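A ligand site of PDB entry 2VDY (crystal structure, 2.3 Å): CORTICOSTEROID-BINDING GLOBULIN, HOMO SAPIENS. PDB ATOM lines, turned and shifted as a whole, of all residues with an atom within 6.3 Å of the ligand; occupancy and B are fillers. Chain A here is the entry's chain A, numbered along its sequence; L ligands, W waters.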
ATOM      1  N   ALA A   8      -7.709 -38.384  23.355  1.00  0.00           N
ATOM      2  CA  ALA A   8      -8.428 -37.113  23.460  1.00  0.00           C
ATOM      3  C   ALA A   8      -9.806 -37.252  24.116  1.00  0.00           C
ATOM      4  O   ALA A   8     -10.224 -36.400  24.902  1.00  0.00           O
ATOM      5  CB  ALA A   8      -8.550 -36.450  22.089  1.00  0.00           C
ATOM      6  N   SER A   9     -10.498 -38.350  23.787  1.00  0.00           N
ATOM      7  CA  SER A   9     -11.813 -38.645  24.359  1.00  0.00           C
ATOM      8  C   SER A   9     -11.702 -39.082  25.817  1.00  0.00           C
ATOM      9  O   SER A   9     -12.495 -38.653  26.664  1.00  0.00           O
ATOM     10  CB  SER A   9     -12.505 -39.731  23.529  1.00  0.00           C
ATOM     11  OG  SER A   9     -13.758 -40.081  24.085  1.00  0.00           O
ATOM     12  N   ALA A  10     -10.726 -39.933  26.104  1.00  0.00           N
ATOM     13  CA  ALA A  10     -10.508 -40.480  27.446  1.00  0.00           C
ATOM     14  C   ALA A  10     -10.030 -39.409  28.426  1.00  0.00           C
ATOM     15  O   ALA A  10     -10.465 -39.395  29.584  1.00  0.00           O
ATOM     16  CB  ALA A  10      -9.509 -41.632  27.385  1.00  0.00           C
ATOM     17  N   VAL A  12     -10.564 -36.073  28.325  1.00  0.00           N
ATOM     18  CA  VAL A  12     -11.592 -35.073  28.640  1.00  0.00           C
ATOM     19  C   VAL A  12     -12.678 -35.654  29.549  1.00  0.00           C
ATOM     20  O   VAL A  12     -13.243 -34.931  30.377  1.00  0.00           O
ATOM     21  CB  VAL A  12     -12.156 -34.373  27.355  1.00  0.00           C
ATOM     22  CG1 VAL A  12     -13.020 -35.305  26.537  1.00  0.00           C
ATOM     23  CG2 VAL A  12     -12.908 -33.099  27.714  1.00  0.00           C
ATOM     24  N   PHE A  16     -13.664 -34.022  33.382  1.00  0.00           N
ATOM     25  CA  PHE A  16     -14.980 -33.693  33.915  1.00  0.00           C
ATOM     26  C   PHE A  16     -15.363 -34.500  35.154  1.00  0.00           C
ATOM     27  O   PHE A  16     -16.003 -33.978  36.072  1.00  0.00           O
ATOM     28  CB  PHE A  16     -16.071 -33.840  32.849  1.00  0.00           C
ATOM     29  CG  PHE A  16     -15.941 -32.877  31.699  1.00  0.00           C
ATOM     30  CD1 PHE A  16     -15.633 -31.537  31.918  1.00  0.00           C
ATOM     31  CD2 PHE A  16     -16.144 -33.310  30.400  1.00  0.00           C
ATOM     32  CE1 PHE A  16     -15.520 -30.642  30.857  1.00  0.00           C
ATOM     33  CE2 PHE A  16     -16.031 -32.424  29.324  1.00  0.00           C
ATOM     34  CZ  PHE A  16     -15.720 -31.096  29.550  1.00  0.00           C
ATOM     35  N   GLN A 222     -17.849 -17.963  24.503  1.00  0.00           N
ATOM     36  CA  GLN A 222     -16.564 -18.548  24.142  1.00  0.00           C
ATOM     37  C   GLN A 222     -15.618 -17.487  23.587  1.00  0.00           C
ATOM     38  O   GLN A 222     -16.000 -16.708  22.709  1.00  0.00           O
ATOM     39  CB  GLN A 222     -16.740 -19.685  23.130  1.00  0.00           C
ATOM     40  CG  GLN A 222     -15.480 -20.545  22.946  1.00  0.00           C
ATOM     41  CD  GLN A 222     -15.597 -21.554  21.805  1.00  0.00           C
ATOM     42  OE1 GLN A 222     -16.655 -21.689  21.180  1.00  0.00           O
ATOM     43  NE2 GLN A 222     -14.515 -22.265  21.536  1.00  0.00           N
ATOM     44  N   THR A 230      -8.407 -21.689  23.717  1.00  0.00           N
ATOM     45  CA  THR A 230      -9.779 -21.175  23.787  1.00  0.00           C
ATOM     46  C   THR A 230     -10.375 -21.373  25.196  1.00  0.00           C
ATOM     47  O   THR A 230      -9.941 -22.255  25.941  1.00  0.00           O
ATOM     48  CB  THR A 230     -10.702 -21.815  22.703  1.00  0.00           C
ATOM     49  OG1 THR A 230     -11.971 -21.145  22.695  1.00  0.00           O
ATOM     50  CG2 THR A 230     -10.900 -23.316  22.942  1.00  0.00           C
ATOM     51  N   PHE A 232     -14.148 -21.217  27.707  1.00  0.00           N
ATOM     52  CA  PHE A 232     -15.584 -21.085  27.938  1.00  0.00           C
ATOM     53  C   PHE A 232     -15.826 -20.484  29.324  1.00  0.00           C
ATOM     54  O   PHE A 232     -15.298 -20.969  30.327  1.00  0.00           O
ATOM     55  CB  PHE A 232     -16.289 -22.446  27.864  1.00  0.00           C
ATOM     56  CG  PHE A 232     -16.227 -23.096  26.510  1.00  0.00           C
ATOM     57  CD1 PHE A 232     -15.169 -23.926  26.168  1.00  0.00           C
ATOM     58  CD2 PHE A 232     -17.254 -22.912  25.593  1.00  0.00           C
ATOM     59  CE1 PHE A 232     -15.119 -24.550  24.924  1.00  0.00           C
ATOM     60  CE2 PHE A 232     -17.218 -23.533  24.346  1.00  0.00           C
ATOM     61  CZ  PHE A 232     -16.141 -24.350  24.005  1.00  0.00           C
ATOM     62  N   ARG A 250     -18.738 -34.400  27.171  1.00  0.00           N
ATOM     63  CA  ARG A 250     -18.436 -34.230  25.753  1.00  0.00           C
ATOM     64  C   ARG A 250     -19.660 -33.821  24.940  1.00  0.00           C
ATOM     65  O   ARG A 250     -19.573 -32.982  24.041  1.00  0.00           O
ATOM     66  CB  ARG A 250     -17.821 -35.499  25.165  1.00  0.00           C
ATOM     67  CG  ARG A 250     -16.330 -35.612  25.352  1.00  0.00           C
ATOM     68  CD  ARG A 250     -15.762 -36.829  24.623  1.00  0.00           C
ATOM     69  NE  ARG A 250     -15.999 -38.072  25.346  1.00  0.00           N
ATOM     70  CZ  ARG A 250     -16.848 -39.029  24.970  1.00  0.00           C
ATOM     71  NH1 ARG A 250     -16.987 -40.126  25.700  1.00  0.00           N
ATOM     72  NH2 ARG A 250     -17.559 -38.897  23.848  1.00  0.00           N
ATOM     73  N   ASP A 251     -20.810 -34.411  25.261  1.00  0.00           N
ATOM     74  CA  ASP A 251     -22.069 -34.119  24.591  1.00  0.00           C
ATOM     75  C   ASP A 251     -22.580 -32.703  24.843  1.00  0.00           C
ATOM     76  O   ASP A 251     -23.198 -32.089  23.972  1.00  0.00           O
ATOM     77  CB  ASP A 251     -23.145 -35.139  24.983  1.00  0.00           C
ATOM     78  CG  ASP A 251     -22.913 -36.496  24.353  1.00  0.00           C
ATOM     79  OD1 ASP A 251     -22.128 -37.292  24.911  1.00  0.00           O
ATOM     80  OD2 ASP A 251     -23.520 -36.773  23.299  1.00  0.00           O
ATOM     81  N   ILE A 253     -20.553 -29.948  25.778  1.00  0.00           N
ATOM     82  CA  ILE A 253     -19.617 -29.010  25.152  1.00  0.00           C
ATOM     83  C   ILE A 253     -19.722 -28.998  23.617  1.00  0.00           C
ATOM     84  O   ILE A 253     -19.491 -27.974  22.988  1.00  0.00           O
ATOM     85  CB  ILE A 253     -18.150 -29.226  25.606  1.00  0.00           C
ATOM     86  CG1 ILE A 253     -17.637 -30.614  25.194  1.00  0.00           C
ATOM     87  CG2 ILE A 253     -18.027 -29.006  27.125  1.00  0.00           C
ATOM     88  CD1 ILE A 253     -16.150 -30.821  25.405  1.00  0.00           C
ATOM     89  N   ASN A 254     -20.071 -30.157  23.042  1.00  0.00           N
ATOM     90  CA  ASN A 254     -20.375 -30.259  21.607  1.00  0.00           C
ATOM     91  C   ASN A 254     -21.615 -29.458  21.231  1.00  0.00           C
ATOM     92  O   ASN A 254     -21.605 -28.720  20.249  1.00  0.00           O
ATOM     93  CB  ASN A 254     -20.574 -31.726  21.196  1.00  0.00           C
ATOM     94  CG  ASN A 254     -19.273 -32.420  20.836  1.00  0.00           C
ATOM     95  OD1 ASN A 254     -18.454 -31.890  20.089  1.00  0.00           O
ATOM     96  ND2 ASN A 254     -19.078 -33.631  21.363  1.00  0.00           N
ATOM     97  N   SER A 257     -20.859 -25.739  21.590  1.00  0.00           N
ATOM     98  CA  SER A 257     -20.067 -25.355  20.422  1.00  0.00           C
ATOM     99  C   SER A 257     -20.943 -25.152  19.175  1.00  0.00           C
ATOM    100  O   SER A 257     -20.766 -24.174  18.438  1.00  0.00           O
ATOM    101  CB  SER A 257     -18.977 -26.397  20.144  1.00  0.00           C
ATOM    102  OG  SER A 257     -18.269 -26.122  18.957  1.00  0.00           O
ATOM    103  N   LEU A 260     -23.407 -22.008  20.048  1.00  0.00           N
ATOM    104  CA  LEU A 260     -22.803 -20.681  20.199  1.00  0.00           C
ATOM    105  C   LEU A 260     -22.879 -19.875  18.908  1.00  0.00           C
ATOM    106  O   LEU A 260     -22.406 -20.314  17.858  1.00  0.00           O
ATOM    107  CB  LEU A 260     -21.350 -20.791  20.673  1.00  0.00           C
ATOM    108  CG  LEU A 260     -21.094 -21.059  22.166  1.00  0.00           C
ATOM    109  CD1 LEU A 260     -19.771 -21.777  22.365  1.00  0.00           C
ATOM    110  CD2 LEU A 260     -21.153 -19.797  22.995  1.00  0.00           C
ATOM    111  N   PHE A 356      -9.465 -24.769  26.948  1.00  0.00           N
ATOM    112  CA  PHE A 356      -9.161 -25.881  26.039  1.00  0.00           C
ATOM    113  C   PHE A 356      -8.116 -25.508  24.987  1.00  0.00           C
ATOM    114  O   PHE A 356      -7.834 -24.331  24.755  1.00  0.00           O
ATOM    115  CB  PHE A 356     -10.428 -26.344  25.322  1.00  0.00           C
ATOM    116  CG  PHE A 356     -11.274 -27.303  26.118  1.00  0.00           C
ATOM    117  CD1 PHE A 356     -12.308 -26.833  26.914  1.00  0.00           C
ATOM    118  CD2 PHE A 356     -11.034 -28.671  26.060  1.00  0.00           C
ATOM    119  CE1 PHE A 356     -13.096 -27.715  27.649  1.00  0.00           C
ATOM    120  CE2 PHE A 356     -11.811 -29.570  26.792  1.00  0.00           C
ATOM    121  CZ  PHE A 356     -12.842 -29.088  27.594  1.00  0.00           C
ATOM    122  N   ASP A 357      -7.557 -26.536  24.352  1.00  0.00           N
ATOM    123  CA  ASP A 357      -6.750 -26.377  23.157  1.00  0.00           C
ATOM    124  C   ASP A 357      -7.554 -26.840  21.952  1.00  0.00           C
ATOM    125  O   ASP A 357      -7.965 -28.006  21.893  1.00  0.00           O
ATOM    126  CB  ASP A 357      -5.442 -27.169  23.272  1.00  0.00           C
ATOM    127  CG  ASP A 357      -4.649 -27.211  21.969  1.00  0.00           C
ATOM    128  OD1 ASP A 357      -4.675 -26.221  21.204  1.00  0.00           O
ATOM    129  OD2 ASP A 357      -3.986 -28.237  21.704  1.00  0.00           O
ATOM    130  N   HIS A 358      -7.783 -25.934  21.000  1.00  0.00           N
ATOM    131  CA  HIS A 358      -8.468 -26.257  19.726  1.00  0.00           C
ATOM    132  C   HIS A 358      -7.807 -27.394  18.961  1.00  0.00           C
ATOM    133  O   HIS A 358      -8.502 -28.205  18.336  1.00  0.00           O
ATOM    134  CB  HIS A 358      -8.516 -25.028  18.809  1.00  0.00           C
ATOM    135  CG  HIS A 358      -9.693 -24.124  19.030  1.00  0.00           C
ATOM    136  ND1 HIS A 358     -10.999 -24.557  18.888  1.00  0.00           N
ATOM    137  CD2 HIS A 358      -9.772 -22.809  19.337  1.00  0.00           C
ATOM    138  CE1 HIS A 358     -11.822 -23.553  19.124  1.00  0.00           C
ATOM    139  NE2 HIS A 358     -11.100 -22.485  19.405  1.00  0.00           N
ATOM    140  N   PHE A 359      -6.478 -27.457  19.013  1.00  0.00           N
ATOM    141  CA  PHE A 359      -5.683 -28.360  18.182  1.00  0.00           C
ATOM    142  C   PHE A 359      -5.744 -29.833  18.618  1.00  0.00           C
ATOM    143  O   PHE A 359      -5.882 -30.725  17.788  1.00  0.00           O
ATOM    144  CB  PHE A 359      -4.232 -27.866  18.102  1.00  0.00           C
ATOM    145  CG  PHE A 359      -3.426 -28.478  16.993  1.00  0.00           C
ATOM    146  CD1 PHE A 359      -2.553 -29.532  17.245  1.00  0.00           C
ATOM    147  CD2 PHE A 359      -3.520 -27.995  15.687  1.00  0.00           C
ATOM    148  CE1 PHE A 359      -1.797 -30.109  16.215  1.00  0.00           C
ATOM    149  CE2 PHE A 359      -2.771 -28.552  14.652  1.00  0.00           C
ATOM    150  CZ  PHE A 359      -1.912 -29.617  14.917  1.00  0.00           C
ATOM    151  N   THR A 360      -5.637 -30.068  19.926  1.00  0.00           N
ATOM    152  CA  THR A 360      -5.587 -31.435  20.471  1.00  0.00           C
ATOM    153  C   THR A 360      -6.853 -31.861  21.206  1.00  0.00           C
ATOM    154  O   THR A 360      -7.024 -33.039  21.533  1.00  0.00           O
ATOM    155  CB  THR A 360      -4.394 -31.622  21.431  1.00  0.00           C
ATOM    156  OG1 THR A 360      -4.540 -30.723  22.536  1.00  0.00           O
ATOM    157  CG2 THR A 360      -3.070 -31.348  20.726  1.00  0.00           C
ATOM    158  N   TRP A 361      -7.739 -30.892  21.474  1.00  0.00           N
ATOM    159  CA  TRP A 361      -8.949 -31.081  22.279  1.00  0.00           C
ATOM    160  C   TRP A 361      -8.674 -31.337  23.772  1.00  0.00           C
ATOM    161  O   TRP A 361      -9.540 -31.842  24.491  1.00  0.00           O
ATOM    162  CB  TRP A 361      -9.851 -32.194  21.711  1.00  0.00           C
ATOM    163  CG  TRP A 361     -10.372 -31.937  20.320  1.00  0.00           C
ATOM    164  CD1 TRP A 361     -10.569 -30.722  19.725  1.00  0.00           C
ATOM    165  CD2 TRP A 361     -10.806 -32.918  19.383  1.00  0.00           C
ATOM    166  NE1 TRP A 361     -11.070 -30.893  18.456  1.00  0.00           N
ATOM    167  CE2 TRP A 361     -11.234 -32.236  18.228  1.00  0.00           C
ATOM    168  CE3 TRP A 361     -10.864 -34.326  19.402  1.00  0.00           C
ATOM    169  CZ2 TRP A 361     -11.725 -32.904  17.093  1.00  0.00           C
ATOM    170  CZ3 TRP A 361     -11.353 -34.981  18.274  1.00  0.00           C
ATOM    171  CH2 TRP A 361     -11.768 -34.271  17.136  1.00  0.00           C
ATOM    172  N   SER A 362      -7.480 -30.968  24.238  1.00  0.00           N
ATOM    173  CA  SER A 362      -7.084 -31.195  25.624  1.00  0.00           C
ATOM    174  C   SER A 362      -7.679 -30.168  26.568  1.00  0.00           C
ATOM    175  O   SER A 362      -7.598 -28.958  26.329  1.00  0.00           O
ATOM    176  CB  SER A 362      -5.561 -31.190  25.760  1.00  0.00           C
ATOM    177  OG  SER A 362      -5.002 -32.345  25.148  1.00  0.00           O
ATOM    178  N   SER A 363      -8.294 -30.662  27.653  1.00  0.00           N
ATOM    179  CA  SER A 363      -8.743 -29.819  28.746  1.00  0.00           C
ATOM    180  C   SER A 363      -7.536 -29.338  29.531  1.00  0.00           C
ATOM    181  O   SER A 363      -6.945 -30.092  30.307  1.00  0.00           O
ATOM    182  CB  SER A 363      -9.712 -30.570  29.664  1.00  0.00           C
ATOM    183  OG  SER A 363     -10.087 -29.770  30.774  1.00  0.00           O
HETATM  184  C1  LIG L   1     -14.245 -33.562  20.414  1.00  0.00           C
HETATM  185  C2  LIG L   1     -14.253 -35.057  20.732  1.00  0.00           C
HETATM  186  C3  LIG L   1     -13.253 -35.337  21.826  1.00  0.00           C
HETATM  187  C4  LIG L   1     -12.778 -34.243  22.701  1.00  0.00           C
HETATM  188  C5  LIG L   1     -13.419 -33.060  22.724  1.00  0.00           C
HETATM  189  C6  LIG L   1     -13.166 -32.142  23.903  1.00  0.00           C
HETATM  190  C7  LIG L   1     -12.856 -30.719  23.425  1.00  0.00           C
HETATM  191  C8  LIG L   1     -13.821 -30.202  22.347  1.00  0.00           C
HETATM  192  C9  LIG L   1     -13.991 -31.203  21.180  1.00  0.00           C
HETATM  193  C10 LIG L   1     -14.380 -32.633  21.629  1.00  0.00           C
HETATM  194  C11 LIG L   1     -14.355 -29.186  19.573  1.00  0.00           C
HETATM  195  C12 LIG L   1     -14.789 -30.613  19.985  1.00  0.00           C
HETATM  196  C13 LIG L   1     -14.245 -28.218  20.762  1.00  0.00           C
HETATM  197  C14 LIG L   1     -13.313 -28.873  21.777  1.00  0.00           C
HETATM  198  C15 LIG L   1     -12.899 -27.736  22.721  1.00  0.00           C
HETATM  199  C16 LIG L   1     -12.914 -26.499  21.807  1.00  0.00           C
HETATM  200  C17 LIG L   1     -13.482 -26.922  20.458  1.00  0.00           C
HETATM  201  C18 LIG L   1     -15.651 -27.924  21.306  1.00  0.00           C
HETATM  202  C19 LIG L   1     -15.809 -32.755  22.184  1.00  0.00           C
HETATM  203  C20 LIG L   1     -14.329 -25.832  19.818  1.00  0.00           C
HETATM  204  C21 LIG L   1     -14.724 -25.925  18.356  1.00  0.00           C
HETATM  205  O1  LIG L   1     -12.839 -36.482  21.997  1.00  0.00           O
HETATM  206  O2  LIG L   1     -16.203 -30.615  20.231  1.00  0.00           O
HETATM  207  O3  LIG L   1     -12.355 -27.186  19.604  1.00  0.00           O
HETATM  208  O4  LIG L   1     -14.681 -24.857  20.464  1.00  0.00           O
HETATM  209  O5  LIG L   1     -14.643 -24.646  17.724  1.00  0.00           O
HETATM  210  O   HOH W   1     -11.932 -28.408  17.204  1.00  0.00           O
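An oxygen (O1) of the ligand sits close to the backbone NH (N) of Ser 9 (3.5 Å).
The side-chain amide nitrogen of Gln 222 sits at hydrogen-bond distance from an oxygen (O4) of the ligand, at 2.8 Å.
O2 of the ligand lies within hydrogen-bond range of OD1 of Asn 254 (2.6 Å).
An oxygen (O3) of the ligand sits at hydrogen-bond distance from a ring nitrogen (ND1) of His 358.
NE of Arg 250 lies within hydrogen-bond range of OG of Ser 9 (3.3 Å).
ND2 of Asn 254 is in hydrogen-bond range of O of Arg 250 (2.8 Å).
The side-chain amide nitrogen (NE2) of Gln 222 sits at hydrogen-bond distance from the side-chain hydroxyl (OG1) of Thr 230, 3.0 Å away.
N of Phe 356 sits at hydrogen-bond distance from O of Thr 230 (2.7 Å).
Residues that only touch the ligand: Trp 361, Ile 253, Ser 257, Phe 356, Ala 8, Phe 232, Thr 230, Val 12 and Arg 250.
Hydrophobic or aromatic side chains within 4 Å of the ligand: Val 12, Phe 232, Ile 253, Phe 356, His 358 and Trp 361.
Water W1 lies within hydrogen-bond range of O3 of the ligand (2.7 Å) and NE1 of Trp 361 (2.9 Å).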
